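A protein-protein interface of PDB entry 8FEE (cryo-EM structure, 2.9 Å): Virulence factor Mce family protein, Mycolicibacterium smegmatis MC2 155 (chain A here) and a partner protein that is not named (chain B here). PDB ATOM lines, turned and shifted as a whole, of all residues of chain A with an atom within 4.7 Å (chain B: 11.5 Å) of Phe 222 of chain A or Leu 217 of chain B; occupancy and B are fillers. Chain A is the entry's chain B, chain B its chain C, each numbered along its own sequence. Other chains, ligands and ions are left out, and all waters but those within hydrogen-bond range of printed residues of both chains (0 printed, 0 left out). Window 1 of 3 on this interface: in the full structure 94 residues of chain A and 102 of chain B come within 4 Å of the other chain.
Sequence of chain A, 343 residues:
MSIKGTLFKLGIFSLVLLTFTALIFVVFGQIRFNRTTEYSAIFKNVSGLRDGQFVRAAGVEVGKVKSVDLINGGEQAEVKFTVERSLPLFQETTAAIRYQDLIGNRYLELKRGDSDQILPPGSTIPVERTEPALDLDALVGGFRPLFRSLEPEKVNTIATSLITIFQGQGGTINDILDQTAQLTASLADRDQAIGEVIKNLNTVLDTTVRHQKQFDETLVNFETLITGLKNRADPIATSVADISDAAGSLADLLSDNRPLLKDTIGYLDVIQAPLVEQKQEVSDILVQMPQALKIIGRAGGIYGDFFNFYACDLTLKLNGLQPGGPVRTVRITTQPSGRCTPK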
ATOM      1  N   THR A 218     -20.296  -8.737  25.355  1.00  0.00           N
ATOM      2  CA  THR A 218     -19.951  -9.522  26.535  1.00  0.00           C
ATOM      3  C   THR A 218     -18.459  -9.817  26.610  1.00  0.00           C
ATOM      4  O   THR A 218     -17.913  -9.898  27.710  1.00  0.00           O
ATOM      5  CB  THR A 218     -20.755 -10.826  26.590  1.00  0.00           C
ATOM      6  OG1 THR A 218     -20.347 -11.586  27.733  1.00  0.00           O
ATOM      7  CG2 THR A 218     -20.529 -11.669  25.355  1.00  0.00           C
ATOM      8  N   LEU A 219     -17.786  -9.980  25.469  1.00  0.00           N
ATOM      9  CA  LEU A 219     -16.345 -10.221  25.495  1.00  0.00           C
ATOM     10  C   LEU A 219     -15.604  -9.031  26.093  1.00  0.00           C
ATOM     11  O   LEU A 219     -14.746  -9.194  26.968  1.00  0.00           O
ATOM     12  CB  LEU A 219     -15.836 -10.525  24.086  1.00  0.00           C
ATOM     13  CG  LEU A 219     -16.442 -11.747  23.395  1.00  0.00           C
ATOM     14  CD1 LEU A 219     -15.767 -11.996  22.058  1.00  0.00           C
ATOM     15  CD2 LEU A 219     -16.341 -12.974  24.283  1.00  0.00           C
ATOM     16  N   VAL A 220     -15.942  -7.818  25.647  1.00  0.00           N
ATOM     17  CA  VAL A 220     -15.294  -6.620  26.174  1.00  0.00           C
ATOM     18  C   VAL A 220     -15.649  -6.417  27.643  1.00  0.00           C
ATOM     19  O   VAL A 220     -14.789  -6.052  28.456  1.00  0.00           O
ATOM     20  CB  VAL A 220     -15.673  -5.393  25.327  1.00  0.00           C
ATOM     21  CG1 VAL A 220     -14.927  -4.160  25.813  1.00  0.00           C
ATOM     22  CG2 VAL A 220     -15.385  -5.655  23.861  1.00  0.00           C
ATOM     23  N   ASN A 221     -16.917  -6.634  28.006  1.00  0.00           N
ATOM     24  CA  ASN A 221     -17.318  -6.465  29.400  1.00  0.00           C
ATOM     25  C   ASN A 221     -16.603  -7.462  30.304  1.00  0.00           C
ATOM     26  O   ASN A 221     -16.140  -7.105  31.394  1.00  0.00           O
ATOM     27  CB  ASN A 221     -18.833  -6.606  29.537  1.00  0.00           C
ATOM     28  CG  ASN A 221     -19.586  -5.495  28.834  1.00  0.00           C
ATOM     29  OD1 ASN A 221     -20.610  -5.733  28.194  1.00  0.00           O
ATOM     30  ND2 ASN A 221     -19.078  -4.273  28.945  1.00  0.00           N
ATOM     31  N   PHE A 222     -16.506  -8.718  29.864  1.00  0.00           N
ATOM     32  CA  PHE A 222     -15.805  -9.739  30.629  1.00  0.00           C
ATOM     33  C   PHE A 222     -14.328  -9.403  30.761  1.00  0.00           C
ATOM     34  O   PHE A 222     -13.740  -9.582  31.832  1.00  0.00           O
ATOM     35  CB  PHE A 222     -15.994 -11.100  29.961  1.00  0.00           C
ATOM     36  CG  PHE A 222     -16.128 -12.241  30.926  1.00  0.00           C
ATOM     37  CD1 PHE A 222     -15.722 -12.110  32.242  1.00  0.00           C
ATOM     38  CD2 PHE A 222     -16.667 -13.447  30.513  1.00  0.00           C
ATOM     39  CE1 PHE A 222     -15.848 -13.161  33.127  1.00  0.00           C
ATOM     40  CE2 PHE A 222     -16.796 -14.502  31.393  1.00  0.00           C
ATOM     41  CZ  PHE A 222     -16.386 -14.359  32.702  1.00  0.00           C
ATOM     42  N   GLU A 223     -13.710  -8.917  29.681  1.00  0.00           N
ATOM     43  CA  GLU A 223     -12.306  -8.523  29.750  1.00  0.00           C
ATOM     44  C   GLU A 223     -12.101  -7.395  30.752  1.00  0.00           C
ATOM     45  O   GLU A 223     -11.151  -7.425  31.541  1.00  0.00           O
ATOM     46  CB  GLU A 223     -11.807  -8.119  28.361  1.00  0.00           C
ATOM     47  CG  GLU A 223     -10.339  -7.700  28.294  1.00  0.00           C
ATOM     48  CD  GLU A 223     -10.119  -6.227  28.583  1.00  0.00           C
ATOM     49  OE1 GLU A 223     -11.103  -5.460  28.547  1.00  0.00           O
ATOM     50  OE2 GLU A 223      -8.963  -5.837  28.851  1.00  0.00           O
ATOM     51  N   THR A 224     -12.984  -6.392  30.735  1.00  0.00           N
ATOM     52  CA  THR A 224     -12.852  -5.284  31.677  1.00  0.00           C
ATOM     53  C   THR A 224     -13.036  -5.757  33.113  1.00  0.00           C
ATOM     54  O   THR A 224     -12.277  -5.361  34.008  1.00  0.00           O
ATOM     55  CB  THR A 224     -13.859  -4.184  31.344  1.00  0.00           C
ATOM     56  OG1 THR A 224     -13.839  -3.927  29.934  1.00  0.00           O
ATOM     57  CG2 THR A 224     -13.511  -2.906  32.088  1.00  0.00           C
ATOM     58  N   LEU A 225     -14.032  -6.615  33.349  1.00  0.00           N
ATOM     59  CA  LEU A 225     -14.274  -7.141  34.690  1.00  0.00           C
ATOM     60  C   LEU A 225     -13.076  -7.939  35.188  1.00  0.00           C
ATOM     61  O   LEU A 225     -12.626  -7.766  36.329  1.00  0.00           O
ATOM     62  CB  LEU A 225     -15.536  -8.003  34.685  1.00  0.00           C
ATOM     63  CG  LEU A 225     -15.738  -8.991  35.834  1.00  0.00           C
ATOM     64  CD1 LEU A 225     -15.947  -8.256  37.146  1.00  0.00           C
ATOM     65  CD2 LEU A 225     -16.909  -9.912  35.539  1.00  0.00           C
ATOM     66  N   ILE A 226     -12.538  -8.814  34.336  1.00  0.00           N
ATOM     67  CA  ILE A 226     -11.434  -9.676  34.739  1.00  0.00           C
ATOM     68  C   ILE A 226     -10.170  -8.857  34.970  1.00  0.00           C
ATOM     69  O   ILE A 226      -9.412  -9.127  35.905  1.00  0.00           O
ATOM     70  CB  ILE A 226     -11.224 -10.788  33.697  1.00  0.00           C
ATOM     71  CG1 ILE A 226     -12.416 -11.744  33.695  1.00  0.00           C
ATOM     72  CG2 ILE A 226      -9.965 -11.559  33.984  1.00  0.00           C
ATOM     73  CD1 ILE A 226     -12.723 -12.333  35.048  1.00  0.00           C
ATOM     74  N   VAL B 206     -16.457 -10.764  14.547  1.00  0.00           N
ATOM     75  CA  VAL B 206     -16.635 -10.391  15.949  1.00  0.00           C
ATOM     76  C   VAL B 206     -15.466 -10.892  16.790  1.00  0.00           C
ATOM     77  O   VAL B 206     -14.927 -10.161  17.631  1.00  0.00           O
ATOM     78  CB  VAL B 206     -17.982 -10.917  16.479  1.00  0.00           C
ATOM     79  CG1 VAL B 206     -18.102 -10.647  17.968  1.00  0.00           C
ATOM     80  CG2 VAL B 206     -19.129 -10.261  15.738  1.00  0.00           C
ATOM     81  N   LEU B 207     -15.057 -12.146  16.577  1.00  0.00           N
ATOM     82  CA  LEU B 207     -13.955 -12.716  17.353  1.00  0.00           C
ATOM     83  C   LEU B 207     -12.640 -11.995  17.077  1.00  0.00           C
ATOM     84  O   LEU B 207     -11.885 -11.685  18.006  1.00  0.00           O
ATOM     85  CB  LEU B 207     -13.814 -14.207  17.053  1.00  0.00           C
ATOM     86  CG  LEU B 207     -14.800 -15.145  17.748  1.00  0.00           C
ATOM     87  CD1 LEU B 207     -14.534 -16.585  17.349  1.00  0.00           C
ATOM     88  CD2 LEU B 207     -14.709 -14.980  19.255  1.00  0.00           C
ATOM     89  N   ARG B 210     -12.135  -8.372  18.560  1.00  0.00           N
ATOM     90  CA  ARG B 210     -11.946  -8.360  20.005  1.00  0.00           C
ATOM     91  C   ARG B 210     -10.870  -9.339  20.463  1.00  0.00           C
ATOM     92  O   ARG B 210     -10.852  -9.719  21.639  1.00  0.00           O
ATOM     93  CB  ARG B 210     -13.270  -8.662  20.707  1.00  0.00           C
ATOM     94  CG  ARG B 210     -14.401  -7.735  20.303  1.00  0.00           C
ATOM     95  CD  ARG B 210     -14.014  -6.282  20.515  1.00  0.00           C
ATOM     96  NE  ARG B 210     -15.072  -5.367  20.110  1.00  0.00           N
ATOM     97  CZ  ARG B 210     -14.990  -4.047  20.189  1.00  0.00           C
ATOM     98  NH1 ARG B 210     -13.906  -3.449  20.655  1.00  0.00           N
ATOM     99  NH2 ARG B 210     -16.021  -3.307  19.791  1.00  0.00           N
ATOM    100  N   SER B 211      -9.975  -9.751  19.561  1.00  0.00           N
ATOM    101  CA  SER B 211      -9.021 -10.813  19.874  1.00  0.00           C
ATOM    102  C   SER B 211      -8.041 -10.406  20.967  1.00  0.00           C
ATOM    103  O   SER B 211      -7.712 -11.217  21.842  1.00  0.00           O
ATOM    104  CB  SER B 211      -8.262 -11.223  18.619  1.00  0.00           C
ATOM    105  OG  SER B 211      -7.366 -12.270  18.926  1.00  0.00           O
ATOM    106  N   THR B 212      -7.544  -9.168  20.922  1.00  0.00           N
ATOM    107  CA  THR B 212      -6.649  -8.695  21.975  1.00  0.00           C
ATOM    108  C   THR B 212      -7.355  -8.697  23.324  1.00  0.00           C
ATOM    109  O   THR B 212      -6.767  -9.077  24.347  1.00  0.00           O
ATOM    110  CB  THR B 212      -6.133  -7.298  21.636  1.00  0.00           C
ATOM    111  OG1 THR B 212      -5.449  -7.334  20.376  1.00  0.00           O
ATOM    112  CG2 THR B 212      -5.174  -6.803  22.706  1.00  0.00           C
ATOM    113  N   GLN B 213      -8.623  -8.281  23.342  1.00  0.00           N
ATOM    114  CA  GLN B 213      -9.410  -8.348  24.567  1.00  0.00           C
ATOM    115  C   GLN B 213      -9.561  -9.786  25.047  1.00  0.00           C
ATOM    116  O   GLN B 213      -9.487 -10.048  26.248  1.00  0.00           O
ATOM    117  CB  GLN B 213     -10.780  -7.707  24.351  1.00  0.00           C
ATOM    118  CG  GLN B 213     -10.780  -6.189  24.440  1.00  0.00           C
ATOM    119  CD  GLN B 213     -10.237  -5.527  23.192  1.00  0.00           C
ATOM    120  OE1 GLN B 213     -10.180  -6.138  22.125  1.00  0.00           O
ATOM    121  NE2 GLN B 213      -9.833  -4.269  23.317  1.00  0.00           N
ATOM    122  N   VAL B 214      -9.775 -10.730  24.124  1.00  0.00           N
ATOM    123  CA  VAL B 214      -9.904 -12.134  24.515  1.00  0.00           C
ATOM    124  C   VAL B 214      -8.610 -12.641  25.142  1.00  0.00           C
ATOM    125  O   VAL B 214      -8.626 -13.331  26.170  1.00  0.00           O
ATOM    126  CB  VAL B 214     -10.321 -12.991  23.304  1.00  0.00           C
ATOM    127  CG1 VAL B 214     -10.302 -14.466  23.663  1.00  0.00           C
ATOM    128  CG2 VAL B 214     -11.702 -12.591  22.825  1.00  0.00           C
ATOM    129  N   ASN B 215      -7.469 -12.303  24.534  1.00  0.00           N
ATOM    130  CA  ASN B 215      -6.180 -12.741  25.063  1.00  0.00           C
ATOM    131  C   ASN B 215      -5.935 -12.173  26.455  1.00  0.00           C
ATOM    132  O   ASN B 215      -5.535 -12.899  27.378  1.00  0.00           O
ATOM    133  CB  ASN B 215      -5.060 -12.330  24.109  1.00  0.00           C
ATOM    134  CG  ASN B 215      -3.685 -12.528  24.709  1.00  0.00           C
ATOM    135  OD1 ASN B 215      -3.380 -13.587  25.256  1.00  0.00           O
ATOM    136  ND2 ASN B 215      -2.846 -11.503  24.617  1.00  0.00           N
ATOM    137  N   GLN B 216      -6.163 -10.867  26.621  1.00  0.00           N
ATOM    138  CA  GLN B 216      -5.946 -10.244  27.921  1.00  0.00           C
ATOM    139  C   GLN B 216      -6.915 -10.796  28.958  1.00  0.00           C
ATOM    140  O   GLN B 216      -6.538 -11.013  30.115  1.00  0.00           O
ATOM    141  CB  GLN B 216      -6.077  -8.727  27.803  1.00  0.00           C
ATOM    142  CG  GLN B 216      -5.255  -7.960  28.818  1.00  0.00           C
ATOM    143  CD  GLN B 216      -5.043  -6.516  28.417  1.00  0.00           C
ATOM    144  OE1 GLN B 216      -5.597  -6.049  27.423  1.00  0.00           O
ATOM    145  NE2 GLN B 216      -4.234  -5.801  29.189  1.00  0.00           N
ATOM    146  N   LEU B 217      -8.161 -11.049  28.549  1.00  0.00           N
ATOM    147  CA  LEU B 217      -9.146 -11.680  29.419  1.00  0.00           C
ATOM    148  C   LEU B 217      -8.641 -13.021  29.927  1.00  0.00           C
ATOM    149  O   LEU B 217      -8.678 -13.292  31.131  1.00  0.00           O
ATOM    150  CB  LEU B 217     -10.463 -11.835  28.651  1.00  0.00           C
ATOM    151  CG  LEU B 217     -11.761 -12.444  29.195  1.00  0.00           C
ATOM    152  CD1 LEU B 217     -12.888 -12.028  28.273  1.00  0.00           C
ATOM    153  CD2 LEU B 217     -11.736 -13.964  29.291  1.00  0.00           C
ATOM    154  N   LEU B 218      -8.165 -13.874  29.017  1.00  0.00           N
ATOM    155  CA  LEU B 218      -7.727 -15.208  29.420  1.00  0.00           C
ATOM    156  C   LEU B 218      -6.513 -15.144  30.342  1.00  0.00           C
ATOM    157  O   LEU B 218      -6.468 -15.844  31.364  1.00  0.00           O
ATOM    158  CB  LEU B 218      -7.425 -16.056  28.186  1.00  0.00           C
ATOM    159  CG  LEU B 218      -8.632 -16.423  27.321  1.00  0.00           C
ATOM    160  CD1 LEU B 218      -8.218 -17.306  26.158  1.00  0.00           C
ATOM    161  CD2 LEU B 218      -9.700 -17.104  28.155  1.00  0.00           C
ATOM    162  N   VAL B 219      -5.524 -14.306  30.013  1.00  0.00           N
ATOM    163  CA  VAL B 219      -4.315 -14.274  30.835  1.00  0.00           C
ATOM    164  C   VAL B 219      -4.608 -13.678  32.212  1.00  0.00           C
ATOM    165  O   VAL B 219      -4.103 -14.165  33.234  1.00  0.00           O
ATOM    166  CB  VAL B 219      -3.165 -13.549  30.105  1.00  0.00           C
ATOM    167  CG1 VAL B 219      -2.886 -14.224  28.773  1.00  0.00           C
ATOM    168  CG2 VAL B 219      -3.462 -12.077  29.892  1.00  0.00           C
ATOM    169  N   ASN B 220      -5.448 -12.637  32.276  1.00  0.00           N
ATOM    170  CA  ASN B 220      -5.782 -12.058  33.569  1.00  0.00           C
ATOM    171  C   ASN B 220      -6.668 -12.991  34.384  1.00  0.00           C
ATOM    172  O   ASN B 220      -6.572 -13.009  35.614  1.00  0.00           O
ATOM    173  CB  ASN B 220      -6.453 -10.698  33.391  1.00  0.00           C
ATOM    174  CG  ASN B 220      -5.535  -9.678  32.754  1.00  0.00           C
ATOM    175  OD1 ASN B 220      -5.937  -8.933  31.863  1.00  0.00           O
ATOM    176  ND2 ASN B 220      -4.285  -9.656  33.194  1.00  0.00           N
ATOM    177  N   ALA B 221      -7.527 -13.773  33.724  1.00  0.00           N
ATOM    178  CA  ALA B 221      -8.301 -14.782  34.435  1.00  0.00           C
ATOM    179  C   ALA B 221      -7.387 -15.837  35.036  1.00  0.00           C
ATOM    180  O   ALA B 221      -7.602 -16.281  36.169  1.00  0.00           O
ATOM    181  CB  ALA B 221      -9.322 -15.422  33.497  1.00  0.00           C
ATOM    182  N   GLN B 222      -6.362 -16.251  34.288  1.00  0.00           N
ATOM    183  CA  GLN B 222      -5.384 -17.192  34.828  1.00  0.00           C
ATOM    184  C   GLN B 222      -4.688 -16.613  36.053  1.00  0.00           C
ATOM    185  O   GLN B 222      -4.558 -17.286  37.083  1.00  0.00           O
ATOM    186  CB  GLN B 222      -4.365 -17.561  33.748  1.00  0.00           C
ATOM    187  CG  GLN B 222      -3.284 -18.534  34.197  1.00  0.00           C
ATOM    188  CD  GLN B 222      -2.051 -17.836  34.743  1.00  0.00           C
ATOM    189  OE1 GLN B 222      -1.918 -16.618  34.641  1.00  0.00           O
ATOM    190  NE2 GLN B 222      -1.148 -18.608  35.334  1.00  0.00           N
ATOM    191  N   THR B 223      -4.239 -15.359  35.959  1.00  0.00           N
ATOM    192  CA  THR B 223      -3.547 -14.733  37.086  1.00  0.00           C
ATOM    193  C   THR B 223      -4.458 -14.624  38.307  1.00  0.00           C
ATOM    194  O   THR B 223      -4.055 -14.950  39.432  1.00  0.00           O
ATOM    195  CB  THR B 223      -3.026 -13.353  36.677  1.00  0.00           C
ATOM    196  OG1 THR B 223      -2.046 -13.499  35.644  1.00  0.00           O
ATOM    197  CG2 THR B 223      -2.395 -12.647  37.865  1.00  0.00           C
ATOM    198  N   LEU B 224      -5.701 -14.181  38.095  1.00  0.00           N
ATOM    199  CA  LEU B 224      -6.645 -14.025  39.196  1.00  0.00           C
ATOM    200  C   LEU B 224      -6.966 -15.363  39.848  1.00  0.00           C
ATOM    201  O   LEU B 224      -6.992 -15.472  41.078  1.00  0.00           O
ATOM    202  CB  LEU B 224      -7.923 -13.352  38.694  1.00  0.00           C
ATOM    203  CG  LEU B 224      -9.137 -13.407  39.622  1.00  0.00           C
ATOM    204  CD1 LEU B 224      -8.933 -12.514  40.835  1.00  0.00           C
ATOM    205  CD2 LEU B 224     -10.404 -13.026  38.874  1.00  0.00           C
ATOM    206  N   LEU B 225      -7.222 -16.392  39.037  1.00  0.00           N
ATOM    207  CA  LEU B 225      -7.535 -17.702  39.594  1.00  0.00           C
ATOM    208  C   LEU B 225      -6.350 -18.275  40.359  1.00  0.00           C
ATOM    209  O   LEU B 225      -6.531 -18.888  41.419  1.00  0.00           O
ATOM    210  CB  LEU B 225      -7.972 -18.652  38.481  1.00  0.00           C
ATOM    211  CG  LEU B 225      -9.428 -18.533  38.033  1.00  0.00           C
ATOM    212  CD1 LEU B 225      -9.697 -19.451  36.856  1.00  0.00           C
ATOM    213  CD2 LEU B 225     -10.364 -18.852  39.186  1.00  0.00           C
ATOM    214  N   ALA B 226      -5.131 -18.085  39.843  1.00  0.00           N
ATOM    215  CA  ALA B 226      -3.945 -18.555  40.552  1.00  0.00           C
ATOM    216  C   ALA B 226      -3.811 -17.868  41.904  1.00  0.00           C
ATOM    217  O   ALA B 226      -3.575 -18.522  42.930  1.00  0.00           O
ATOM    218  CB  ALA B 226      -2.697 -18.322  39.701  1.00  0.00           C
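Printed residues of chain A that touch a printed residue of chain B: Leu 219, Val 220, Phe 222, Glu 223 and Ile 226. Hydrophobic or aromatic side chains of chain A that line the printed part of chain B: Val 220, Phe 222 and Ile 226. Along chain B the printed residues that touch a printed residue of chain A span positions 210 to 221. Among the printed residues, 9 pairs touch across the chains. Among the printed residues, no Asp or Glu carboxylate lies within 4 Å of a Lys or Arg side-chain nitrogen of the other chain.
Phe 222 of chain A touches one residue of chain B. Of chain A, only Leu 219 (3.6 Å), Phe 222 (3.7 Å), Glu 223 (3.5 Å) and Ile 226 (3.6 Å) come within 4 Å of Leu 217 of chain B. No residue of chain B comes within 4 Å of Thr 218 of chain A. Of chain B, only Leu 217 comes within 4 Å of Leu 219 of chain A. Of chain B, only Gln 213 (3.2 Å), Gln 216 (3.7 Å) and Leu 217 (3.5 Å) come within 4 Å of Glu 223 of chain A. No residue of chain B comes within 4 Å of Leu 225 of chain A. Of chain B, only Leu 217 (3.6 Å), Asn 220 (3.6 Å) and Ala 221 (3.3 Å) come within 4 Å of Ile 226 of chain A. Printed residues of chain A within 4 Å of Ala 221 of chain B: Ile 226 (3.3 Å). Of the printed residues of chain A, Gln 213 of chain B touches Glu 223 (3.2 Å). Printed residues of chain A within 4 Å of Asn 220 of chain B: Ile 226 (3.6 Å). Val 206 of chain B touches none of the printed residues of chain A. The nearest printed residue of chain A that does not touch Ala 221 of chain B is Phe 222 of chain A (6.9 Å).
O of Val 220 of chain A is in hydrogen-bond range of OG1 of Thr 224 of chain A (2.8 Å). The side-chain hydroxyl (OG1) of Thr 224 of chain A is in hydrogen-bond range of the side-chain carboxylate (OE1) of Glu 223 of chain A (3.4 Å). The side-chain amide oxygen (OD1) of Asn 220 of chain B sits close to the backbone carbonyl oxygen (O) of Gln 216 of chain B, 2.8 Å away.
Among the printed residues, merely in contact across the chains: Leu 219 of chain A with Leu 217 of chain B (3.6 Å), Val 220 of chain A with Arg 210 of chain B (3.7 Å), Phe 222 of chain A with Leu 217 of chain B (3.7 Å), Glu 223 of chain A with Gln 213 of chain B (3.2 Å), Glu 223 of chain A with Gln 216 of chain B (3.7 Å), Glu 223 of chain A with Leu 217 of chain B (3.5 Å), Ile 226 of chain A with Leu 217 of chain B (3.6 Å), Ile 226 of chain A with Asn 220 of chain B (3.6 Å) and Ile 226 of chain A with Ala 221 of chain B (3.3 Å).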
